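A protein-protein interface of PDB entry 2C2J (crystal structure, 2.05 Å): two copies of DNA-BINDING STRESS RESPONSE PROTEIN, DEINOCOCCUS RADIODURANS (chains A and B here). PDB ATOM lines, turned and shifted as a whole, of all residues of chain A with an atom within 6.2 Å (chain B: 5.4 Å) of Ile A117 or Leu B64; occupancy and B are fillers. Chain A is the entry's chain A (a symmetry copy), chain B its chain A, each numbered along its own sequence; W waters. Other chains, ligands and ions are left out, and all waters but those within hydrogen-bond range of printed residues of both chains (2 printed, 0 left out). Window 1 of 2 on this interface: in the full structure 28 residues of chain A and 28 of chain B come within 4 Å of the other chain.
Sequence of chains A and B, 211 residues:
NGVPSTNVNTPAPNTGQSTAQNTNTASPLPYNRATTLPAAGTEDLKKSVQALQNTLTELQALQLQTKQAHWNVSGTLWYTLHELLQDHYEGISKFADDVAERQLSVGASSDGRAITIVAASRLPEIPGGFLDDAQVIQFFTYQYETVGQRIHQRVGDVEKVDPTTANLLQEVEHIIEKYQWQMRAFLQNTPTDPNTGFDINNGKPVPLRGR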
ATOM      1  N   THR A  57       9.602   4.047 -11.050  1.00  0.00           N
ATOM      2  CA  THR A  57      10.825   4.374 -11.805  1.00  0.00           C
ATOM      3  C   THR A  57      10.875   5.782 -12.389  1.00  0.00           C
ATOM      4  O   THR A  57      11.907   6.446 -12.289  1.00  0.00           O
ATOM      5  CB  THR A  57      11.104   3.297 -12.907  1.00  0.00           C
ATOM      6  OG1 THR A  57      11.235   2.046 -12.244  1.00  0.00           O
ATOM      7  CG2 THR A  57      12.427   3.596 -13.640  1.00  0.00           C
ATOM      8  N   GLN A  60      11.418   8.255  -9.538  1.00  0.00           N
ATOM      9  CA  GLN A  60      12.822   8.170  -9.101  1.00  0.00           C
ATOM     10  C   GLN A  60      13.764   8.861 -10.070  1.00  0.00           C
ATOM     11  O   GLN A  60      14.737   9.506  -9.662  1.00  0.00           O
ATOM     12  CB  GLN A  60      13.248   6.716  -8.941  1.00  0.00           C
ATOM     13  CG  GLN A  60      12.585   6.056  -7.760  1.00  0.00           C
ATOM     14  CD  GLN A  60      13.202   4.723  -7.484  1.00  0.00           C
ATOM     15  OE1 GLN A  60      13.094   3.789  -8.281  1.00  0.00           O
ATOM     16  NE2 GLN A  60      13.872   4.620  -6.360  1.00  0.00           N
ATOM     17  N   ALA A  61      13.483   8.730 -11.362  1.00  0.00           N
ATOM     18  CA  ALA A  61      14.254   9.456 -12.389  1.00  0.00           C
ATOM     19  C   ALA A  61      14.097  10.965 -12.199  1.00  0.00           C
ATOM     20  O   ALA A  61      15.089  11.698 -12.222  1.00  0.00           O
ATOM     21  CB  ALA A  61      13.815   9.035 -13.826  1.00  0.00           C
ATOM     22  N   GLN A  63      13.197  12.429  -9.387  1.00  0.00           N
ATOM     23  CA  GLN A  63      13.899  12.752  -8.120  1.00  0.00           C
ATOM     24  C   GLN A  63      15.329  13.191  -8.363  1.00  0.00           C
ATOM     25  O   GLN A  63      15.758  14.282  -7.921  1.00  0.00           O
ATOM     26  CB  GLN A  63      13.964  11.514  -7.248  1.00  0.00           C
ATOM     27  CG  GLN A  63      12.997  11.453  -6.118  1.00  0.00           C
ATOM     28  CD  GLN A  63      13.264  10.279  -5.194  1.00  0.00           C
ATOM     29  OE1 GLN A  63      13.433   9.137  -5.648  1.00  0.00           O
ATOM     30  NE2 GLN A  63      13.216  10.534  -3.881  1.00  0.00           N
ATOM     31  N   LEU A  64      16.084  12.325  -9.074  1.00  0.00           N
ATOM     32  CA  LEU A  64      17.471  12.591  -9.364  1.00  0.00           C
ATOM     33  C   LEU A  64      17.671  13.766 -10.272  1.00  0.00           C
ATOM     34  O   LEU A  64      18.608  14.539 -10.067  1.00  0.00           O
ATOM     35  CB  LEU A  64      18.201  11.331  -9.941  1.00  0.00           C
ATOM     36  CG  LEU A  64      18.372  10.185  -8.939  1.00  0.00           C
ATOM     37  CD1 LEU A  64      18.729   8.846  -9.705  1.00  0.00           C
ATOM     38  CD2 LEU A  64      19.407  10.536  -7.901  1.00  0.00           C
ATOM     39  N   ASP A 111      10.834  -2.367  -7.071  1.00  0.00           N
ATOM     40  CA  ASP A 111      12.217  -2.264  -7.582  1.00  0.00           C
ATOM     41  C   ASP A 111      12.622  -0.799  -7.747  1.00  0.00           C
ATOM     42  O   ASP A 111      12.301  -0.160  -8.752  1.00  0.00           O
ATOM     43  CB  ASP A 111      12.448  -3.074  -8.893  1.00  0.00           C
ATOM     44  CG  ASP A 111      13.921  -3.141  -9.283  1.00  0.00           C
ATOM     45  OD1 ASP A 111      14.721  -2.343  -8.765  1.00  0.00           O
ATOM     46  OD2 ASP A 111      14.297  -3.988 -10.134  1.00  0.00           O
ATOM     47  N   GLY A 112      13.354  -0.297  -6.755  1.00  0.00           N
ATOM     48  CA  GLY A 112      13.765   1.097  -6.723  1.00  0.00           C
ATOM     49  C   GLY A 112      15.250   1.286  -6.901  1.00  0.00           C
ATOM     50  O   GLY A 112      15.801   2.319  -6.492  1.00  0.00           O
ATOM     51  N   ARG A 113      15.912   0.289  -7.509  1.00  0.00           N
ATOM     52  CA  ARG A 113      17.386   0.289  -7.608  1.00  0.00           C
ATOM     53  C   ARG A 113      17.895   1.196  -8.708  1.00  0.00           C
ATOM     54  O   ARG A 113      17.193   1.437  -9.691  1.00  0.00           O
ATOM     55  CB  ARG A 113      17.924  -1.138  -7.813  1.00  0.00           C
ATOM     56  CG  ARG A 113      17.537  -2.084  -6.680  1.00  0.00           C
ATOM     57  CD  ARG A 113      17.776  -3.532  -7.036  1.00  0.00           C
ATOM     58  NE  ARG A 113      17.026  -3.965  -8.230  1.00  0.00           N
ATOM     59  CZ  ARG A 113      17.509  -4.834  -9.109  1.00  0.00           C
ATOM     60  NH1 ARG A 113      18.707  -5.355  -8.894  1.00  0.00           N
ATOM     61  NH2 ARG A 113      16.805  -5.210 -10.169  1.00  0.00           N
ATOM     62  N   ALA A 114      19.118   1.691  -8.542  1.00  0.00           N
ATOM     63  CA  ALA A 114      19.710   2.604  -9.531  1.00  0.00           C
ATOM     64  C   ALA A 114      19.780   1.984 -10.945  1.00  0.00           C
ATOM     65  O   ALA A 114      19.530   2.659 -11.971  1.00  0.00           O
ATOM     66  CB  ALA A 114      21.103   2.979  -9.098  1.00  0.00           C
ATOM     67  N   ILE A 115      20.136   0.701 -10.990  1.00  0.00           N
ATOM     68  CA  ILE A 115      20.204  -0.004 -12.296  1.00  0.00           C
ATOM     69  C   ILE A 115      18.827   0.038 -13.001  1.00  0.00           C
ATOM     70  O   ILE A 115      18.742   0.236 -14.217  1.00  0.00           O
ATOM     71  CB  ILE A 115      20.768  -1.482 -12.166  1.00  0.00           C
ATOM     72  CG1 ILE A 115      20.964  -2.075 -13.571  1.00  0.00           C
ATOM     73  CG2 ILE A 115      19.911  -2.402 -11.234  1.00  0.00           C
ATOM     74  CD1 ILE A 115      21.932  -1.198 -14.418  1.00  0.00           C
ATOM     75  N   THR A 116      17.738  -0.071 -12.224  1.00  0.00           N
ATOM     76  CA  THR A 116      16.406  -0.108 -12.795  1.00  0.00           C
ATOM     77  C   THR A 116      15.990   1.270 -13.330  1.00  0.00           C
ATOM     78  O   THR A 116      15.313   1.417 -14.374  1.00  0.00           O
ATOM     79  CB  THR A 116      15.429  -0.604 -11.727  1.00  0.00           C
ATOM     80  OG1 THR A 116      15.876  -1.884 -11.252  1.00  0.00           O
ATOM     81  CG2 THR A 116      14.024  -0.696 -12.253  1.00  0.00           C
ATOM     82  N   ILE A 117      16.381   2.301 -12.596  1.00  0.00           N
ATOM     83  CA  ILE A 117      16.189   3.649 -13.053  1.00  0.00           C
ATOM     84  C   ILE A 117      16.911   3.855 -14.391  1.00  0.00           C
ATOM     85  O   ILE A 117      16.331   4.402 -15.341  1.00  0.00           O
ATOM     86  CB  ILE A 117      16.720   4.687 -12.029  1.00  0.00           C
ATOM     87  CG1 ILE A 117      15.935   4.609 -10.711  1.00  0.00           C
ATOM     88  CG2 ILE A 117      16.593   6.069 -12.644  1.00  0.00           C
ATOM     89  CD1 ILE A 117      16.627   5.389  -9.530  1.00  0.00           C
ATOM     90  N   VAL A 118      18.181   3.451 -14.462  1.00  0.00           N
ATOM     91  CA  VAL A 118      18.901   3.595 -15.758  1.00  0.00           C
ATOM     92  C   VAL A 118      18.253   2.731 -16.866  1.00  0.00           C
ATOM     93  O   VAL A 118      17.985   3.235 -17.938  1.00  0.00           O
ATOM     94  CB  VAL A 118      20.430   3.309 -15.654  1.00  0.00           C
ATOM     95  CG1 VAL A 118      21.043   3.116 -17.090  1.00  0.00           C
ATOM     96  CG2 VAL A 118      21.157   4.464 -14.908  1.00  0.00           C
ATOM     97  N   ALA A 119      17.977   1.468 -16.562  1.00  0.00           N
ATOM     98  CA  ALA A 119      17.393   0.496 -17.511  1.00  0.00           C
ATOM     99  C   ALA A 119      16.043   0.913 -18.017  1.00  0.00           C
ATOM    100  O   ALA A 119      15.773   0.936 -19.225  1.00  0.00           O
ATOM    101  CB  ALA A 119      17.229  -0.849 -16.837  1.00  0.00           C
ATOM    102  N   ALA A 120      15.165   1.222 -17.068  1.00  0.00           N
ATOM    103  CA  ALA A 120      13.758   1.324 -17.377  1.00  0.00           C
ATOM    104  C   ALA A 120      13.506   2.780 -17.627  1.00  0.00           C
ATOM    105  O   ALA A 120      12.564   3.373 -17.107  1.00  0.00           O
ATOM    106  CB  ALA A 120      12.895   0.712 -16.242  1.00  0.00           C
ATOM    107  N   SER A 121      14.403   3.324 -18.459  1.00  0.00           N
ATOM    108  CA  SER A 121      14.424   4.698 -18.959  1.00  0.00           C
ATOM    109  C   SER A 121      13.096   5.102 -19.588  1.00  0.00           C
ATOM    110  O   SER A 121      12.138   5.440 -18.875  1.00  0.00           O
ATOM    111  CB  SER A 121      15.606   4.864 -19.946  1.00  0.00           C
ATOM    112  OG  SER A 121      15.722   6.181 -20.523  1.00  0.00           O
ATOM    113  N   LEU B  59      27.193   8.033  -1.656  1.00  0.00           N
ATOM    114  CA  LEU B  59      26.045   8.341  -0.735  1.00  0.00           C
ATOM    115  C   LEU B  59      24.755   8.130  -1.487  1.00  0.00           C
ATOM    116  O   LEU B  59      23.780   7.606  -0.950  1.00  0.00           O
ATOM    117  CB  LEU B  59      26.120   9.817  -0.235  1.00  0.00           C
ATOM    118  CG  LEU B  59      27.274  10.058   0.746  1.00  0.00           C
ATOM    119  CD1 LEU B  59      27.546  11.562   0.976  1.00  0.00           C
ATOM    120  CD2 LEU B  59      27.127   9.320   2.077  1.00  0.00           C
ATOM    121  N   GLN B  60      24.752   8.550  -2.752  1.00  0.00           N
ATOM    122  CA  GLN B  60      23.566   8.365  -3.606  1.00  0.00           C
ATOM    123  C   GLN B  60      23.251   6.898  -3.835  1.00  0.00           C
ATOM    124  O   GLN B  60      22.082   6.495  -3.868  1.00  0.00           O
ATOM    125  CB  GLN B  60      23.761   9.051  -4.952  1.00  0.00           C
ATOM    126  CG  GLN B  60      23.743  10.552  -4.833  1.00  0.00           C
ATOM    127  CD  GLN B  60      23.689  11.189  -6.185  1.00  0.00           C
ATOM    128  OE1 GLN B  60      24.629  11.094  -6.977  1.00  0.00           O
ATOM    129  NE2 GLN B  60      22.583  11.833  -6.474  1.00  0.00           N
ATOM    130  N   ALA B  61      24.292   6.088  -3.996  1.00  0.00           N
ATOM    131  CA  ALA B  61      24.114   4.628  -4.102  1.00  0.00           C
ATOM    132  C   ALA B  61      23.499   4.075  -2.817  1.00  0.00           C
ATOM    133  O   ALA B  61      22.549   3.290  -2.873  1.00  0.00           O
ATOM    134  CB  ALA B  61      25.469   3.916  -4.413  1.00  0.00           C
ATOM    135  N   LEU B  62      24.065   4.464  -1.675  1.00  0.00           N
ATOM    136  CA  LEU B  62      23.499   4.125  -0.361  1.00  0.00           C
ATOM    137  C   LEU B  62      22.070   4.640  -0.152  1.00  0.00           C
ATOM    138  O   LEU B  62      21.257   3.956   0.438  1.00  0.00           O
ATOM    139  CB  LEU B  62      24.408   4.633   0.777  1.00  0.00           C
ATOM    140  CG  LEU B  62      25.710   3.824   0.924  1.00  0.00           C
ATOM    141  CD1 LEU B  62      26.598   4.489   1.950  1.00  0.00           C
ATOM    142  CD2 LEU B  62      25.462   2.375   1.296  1.00  0.00           C
ATOM    143  N   GLN B  63      21.784   5.847  -0.631  1.00  0.00           N
ATOM    144  CA  GLN B  63      20.397   6.372  -0.589  1.00  0.00           C
ATOM    145  C   GLN B  63      19.404   5.392  -1.180  1.00  0.00           C
ATOM    146  O   GLN B  63      18.404   5.009  -0.531  1.00  0.00           O
ATOM    147  CB  GLN B  63      20.310   7.638  -1.418  1.00  0.00           C
ATOM    148  CG  GLN B  63      20.290   8.920  -0.662  1.00  0.00           C
ATOM    149  CD  GLN B  63      20.008  10.113  -1.557  1.00  0.00           C
ATOM    150  OE1 GLN B  63      20.632  10.274  -2.618  1.00  0.00           O
ATOM    151  NE2 GLN B  63      19.127  11.007  -1.094  1.00  0.00           N
ATOM    152  N   LEU B  64      19.679   4.983  -2.438  1.00  0.00           N
ATOM    153  CA  LEU B  64      18.813   4.072  -3.145  1.00  0.00           C
ATOM    154  C   LEU B  64      18.769   2.705  -2.533  1.00  0.00           C
ATOM    155  O   LEU B  64      17.699   2.097  -2.484  1.00  0.00           O
ATOM    156  CB  LEU B  64      19.180   3.974  -4.664  1.00  0.00           C
ATOM    157  CG  LEU B  64      18.904   5.251  -5.465  1.00  0.00           C
ATOM    158  CD1 LEU B  64      19.672   5.198  -6.849  1.00  0.00           C
ATOM    159  CD2 LEU B  64      17.422   5.453  -5.648  1.00  0.00           C
ATOM    160  N   GLN B  65      19.908   2.206  -2.064  1.00  0.00           N
ATOM    161  CA  GLN B  65      19.913   0.889  -1.408  1.00  0.00           C
ATOM    162  C   GLN B  65      19.201   0.836  -0.055  1.00  0.00           C
ATOM    163  O   GLN B  65      18.529  -0.167   0.260  1.00  0.00           O
ATOM    164  CB  GLN B  65      21.348   0.340  -1.263  1.00  0.00           C
ATOM    165  CG  GLN B  65      21.951  -0.024  -2.677  1.00  0.00           C
ATOM    166  CD  GLN B  65      23.429  -0.060  -2.676  1.00  0.00           C
ATOM    167  OE1 GLN B  65      24.071   0.154  -1.634  1.00  0.00           O
ATOM    168  NE2 GLN B  65      24.016  -0.308  -3.863  1.00  0.00           N
ATOM    169  N   THR B  66      19.438   1.832   0.791  1.00  0.00           N
ATOM    170  CA  THR B  66      18.683   1.860   2.073  1.00  0.00           C
ATOM    171  C   THR B  66      17.166   1.935   1.825  1.00  0.00           C
ATOM    172  O   THR B  66      16.389   1.274   2.504  1.00  0.00           O
ATOM    173  CB  THR B  66      19.112   3.018   3.016  1.00  0.00           C
ATOM    174  OG1 THR B  66      19.029   4.278   2.340  1.00  0.00           O
ATOM    175  CG2 THR B  66      20.546   2.825   3.515  1.00  0.00           C
ATOM    176  N   LYS B  67      16.734   2.751   0.876  1.00  0.00           N
ATOM    177  CA  LYS B  67      15.305   2.841   0.626  1.00  0.00           C
ATOM    178  C   LYS B  67      14.741   1.492   0.062  1.00  0.00           C
ATOM    179  O   LYS B  67      13.666   1.008   0.478  1.00  0.00           O
ATOM    180  CB  LYS B  67      15.022   4.008  -0.319  1.00  0.00           C
ATOM    181  CG  LYS B  67      13.533   4.245  -0.550  1.00  0.00           C
ATOM    182  CD  LYS B  67      12.821   4.714   0.760  1.00  0.00           C
ATOM    183  CE  LYS B  67      13.383   6.077   1.163  1.00  0.00           C
ATOM    184  NZ  LYS B  67      12.316   7.052   1.411  1.00  0.00           N
ATOM    185  N   GLN B  68      15.483   0.869  -0.853  1.00  0.00           N
ATOM    186  CA  GLN B  68      15.051  -0.426  -1.396  1.00  0.00           C
ATOM    187  C   GLN B  68      14.884  -1.469  -0.290  1.00  0.00           C
ATOM    188  O   GLN B  68      13.867  -2.159  -0.199  1.00  0.00           O
ATOM    189  CB  GLN B  68      16.111  -0.917  -2.405  1.00  0.00           C
ATOM    190  CG  GLN B  68      15.847  -2.295  -2.943  1.00  0.00           C
ATOM    191  CD  GLN B  68      14.780  -2.260  -3.989  1.00  0.00           C
ATOM    192  OE1 GLN B  68      14.318  -1.171  -4.386  1.00  0.00           O
ATOM    193  NE2 GLN B  68      14.362  -3.436  -4.456  1.00  0.00           N
ATOM    194  N   ALA B  69      15.888  -1.560   0.561  1.00  0.00           N
ATOM    195  CA  ALA B  69      15.846  -2.437   1.718  1.00  0.00           C
ATOM    196  C   ALA B  69      14.699  -2.072   2.684  1.00  0.00           C
ATOM    197  O   ALA B  69      13.983  -2.955   3.159  1.00  0.00           O
ATOM    198  CB  ALA B  69      17.203  -2.408   2.431  1.00  0.00           C
ATOM    199  N   TYR B  89      18.565   6.421   5.776  1.00  0.00           N
ATOM    200  CA  TYR B  89      18.245   7.137   4.520  1.00  0.00           C
ATOM    201  C   TYR B  89      18.267   8.659   4.727  1.00  0.00           C
ATOM    202  O   TYR B  89      18.862   9.427   3.945  1.00  0.00           O
ATOM    203  CB  TYR B  89      16.881   6.680   3.990  1.00  0.00           C
ATOM    204  CG  TYR B  89      16.484   7.393   2.737  1.00  0.00           C
ATOM    205  CD1 TYR B  89      16.953   6.936   1.487  1.00  0.00           C
ATOM    206  CD2 TYR B  89      15.675   8.550   2.782  1.00  0.00           C
ATOM    207  CE1 TYR B  89      16.574   7.585   0.289  1.00  0.00           C
ATOM    208  CE2 TYR B  89      15.298   9.229   1.592  1.00  0.00           C
ATOM    209  CZ  TYR B  89      15.769   8.733   0.348  1.00  0.00           C
ATOM    210  OH  TYR B  89      15.436   9.354  -0.833  1.00  0.00           O
ATOM    211  N   ALA B 114      21.554   9.542 -12.352  1.00  0.00           N
ATOM    212  CA  ALA B 114      21.399   8.088 -12.198  1.00  0.00           C
ATOM    213  C   ALA B 114      22.474   7.291 -12.972  1.00  0.00           C
ATOM    214  O   ALA B 114      23.007   6.265 -12.487  1.00  0.00           O
ATOM    215  CB  ALA B 114      20.039   7.672 -12.694  1.00  0.00           C
ATOM    216  N   ILE B 117      25.667   7.228 -10.928  1.00  0.00           N
ATOM    217  CA  ILE B 117      25.540   6.276  -9.861  1.00  0.00           C
ATOM    218  C   ILE B 117      25.796   4.859 -10.392  1.00  0.00           C
ATOM    219  O   ILE B 117      26.557   4.088  -9.788  1.00  0.00           O
ATOM    220  CB  ILE B 117      24.132   6.323  -9.210  1.00  0.00           C
ATOM    221  CG1 ILE B 117      23.880   7.684  -8.545  1.00  0.00           C
ATOM    222  CG2 ILE B 117      24.045   5.205  -8.185  1.00  0.00           C
ATOM    223  CD1 ILE B 117      22.370   7.917  -8.162  1.00  0.00           C
HETATM  224  O   HOH W   1      20.604  14.044  -8.250  1.00  0.00           O
HETATM  225  O   HOH W   2      15.423   2.937  -3.768  1.00  0.00           O
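The side-chain amide oxygen (OE1) of Gln B68 is in hydrogen-bond range of the backbone NH (N) of Gly A112 (2.7 Å).
The side-chain amide nitrogen (NE2) of Gln A60 lies within hydrogen-bond range of the backbone carbonyl oxygen (O) of Gly A112, 3.0 Å away. NH2 of Arg A113 lies within salt-bridge range of OD2 of Asp A111 (2.8 Å). The side-chain hydroxyl of Thr A116 sits at hydrogen-bond distance from the side-chain carboxylate of Asp A111 (2.8 Å).
Among the printed residues, merely in contact across the chains: Leu A64 with Ala B114 (3.5 Å), Ala A114 with Leu B64 (3.5 Å), Val A118 with Ala B114 (3.5 Å), Gly A112 with Leu B64 (3.6 Å), Gln A60 with Leu B64 (3.7 Å), Leu A64 with Gln B60 (3.7 Å), Asp A111 with Gln B68 (3.8 Å), Arg A113 with Gln B68 (3.8 Å), Ala A114 with Ile B117 (3.8 Å), Ile A117 with Ala B114 (3.8 Å), Gln A63 with Tyr B89 (3.95 Å), Ile A117 with Leu B64 (3.96 Å) and Leu A64 with Ile B117 (3.96 Å).
Of the printed residues of chain B, Gln A63 touches Tyr B89. Of the printed residues of chain B, Leu A64 touches Gln B60 (3.7 Å), Ala B114 (3.5 Å) and Ile B117 (3.96 Å). Of the printed residues of chain B, Asp A111 touches Gln B68. Of the printed residues of chain B, Arg A113 touches Gln B68 (3.8 Å). Ile A117 touches just these residues of chain B: Leu B64 (3.96 Å) and Ala B114 (3.8 Å). The nearest printed residue of chain B that does not touch Ile A117 is Ile B117 (6.4 Å). The nearest printed residue of chain A that does not touch Leu B64 is Leu A64 (4.7 Å). The nearest printed residue of chain B that does not touch Arg A113 is Leu B64 (4.8 Å).
Of the 16 printed residues of chain A, 9 touch a printed residue of chain B. Printed residues of chain A that touch a printed residue of chain B: Gln A60, Gln A63, Leu A64, Asp A111, Gly A112, Arg A113, Ala A114, Ile A117 and Val A118. Hydrophobic or aromatic side chains of chain A within 4 Å of the printed part of chain B: Leu A64, Ala A114, Ile A117 and Val A118. Of the 14 printed residues of chain B, 6 touch a printed residue of chain A. Hydrophobic or aromatic side chains of chain B that line the printed part of chain A: Leu B64, Tyr B89, Ala B114 and Ile B117.
Gln A60 touches Leu B64, and with the chains exchanged Leu A64 touches Gln B60. Leu A64 touches Ala B114, and with the chains exchanged Ala A114 touches Leu B64. Leu A64 touches Ile B117, and with the chains exchanged Ile A117 touches Leu B64. Ala A114 touches Ile B117, and with the chains exchanged Ile A117 touches Ala B114. 6 positions are printed for both chains.
Water W2 lies within hydrogen-bond range of the backbone carbonyl oxygen of Leu B64 (2.7 Å), the backbone carbonyl oxygen of Gly A112 (2.8 Å) and the side-chain amide nitrogen of Gln A60 (3.5 Å). Water W1 bridges O of Leu A64 and NE2 of Gln B60.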
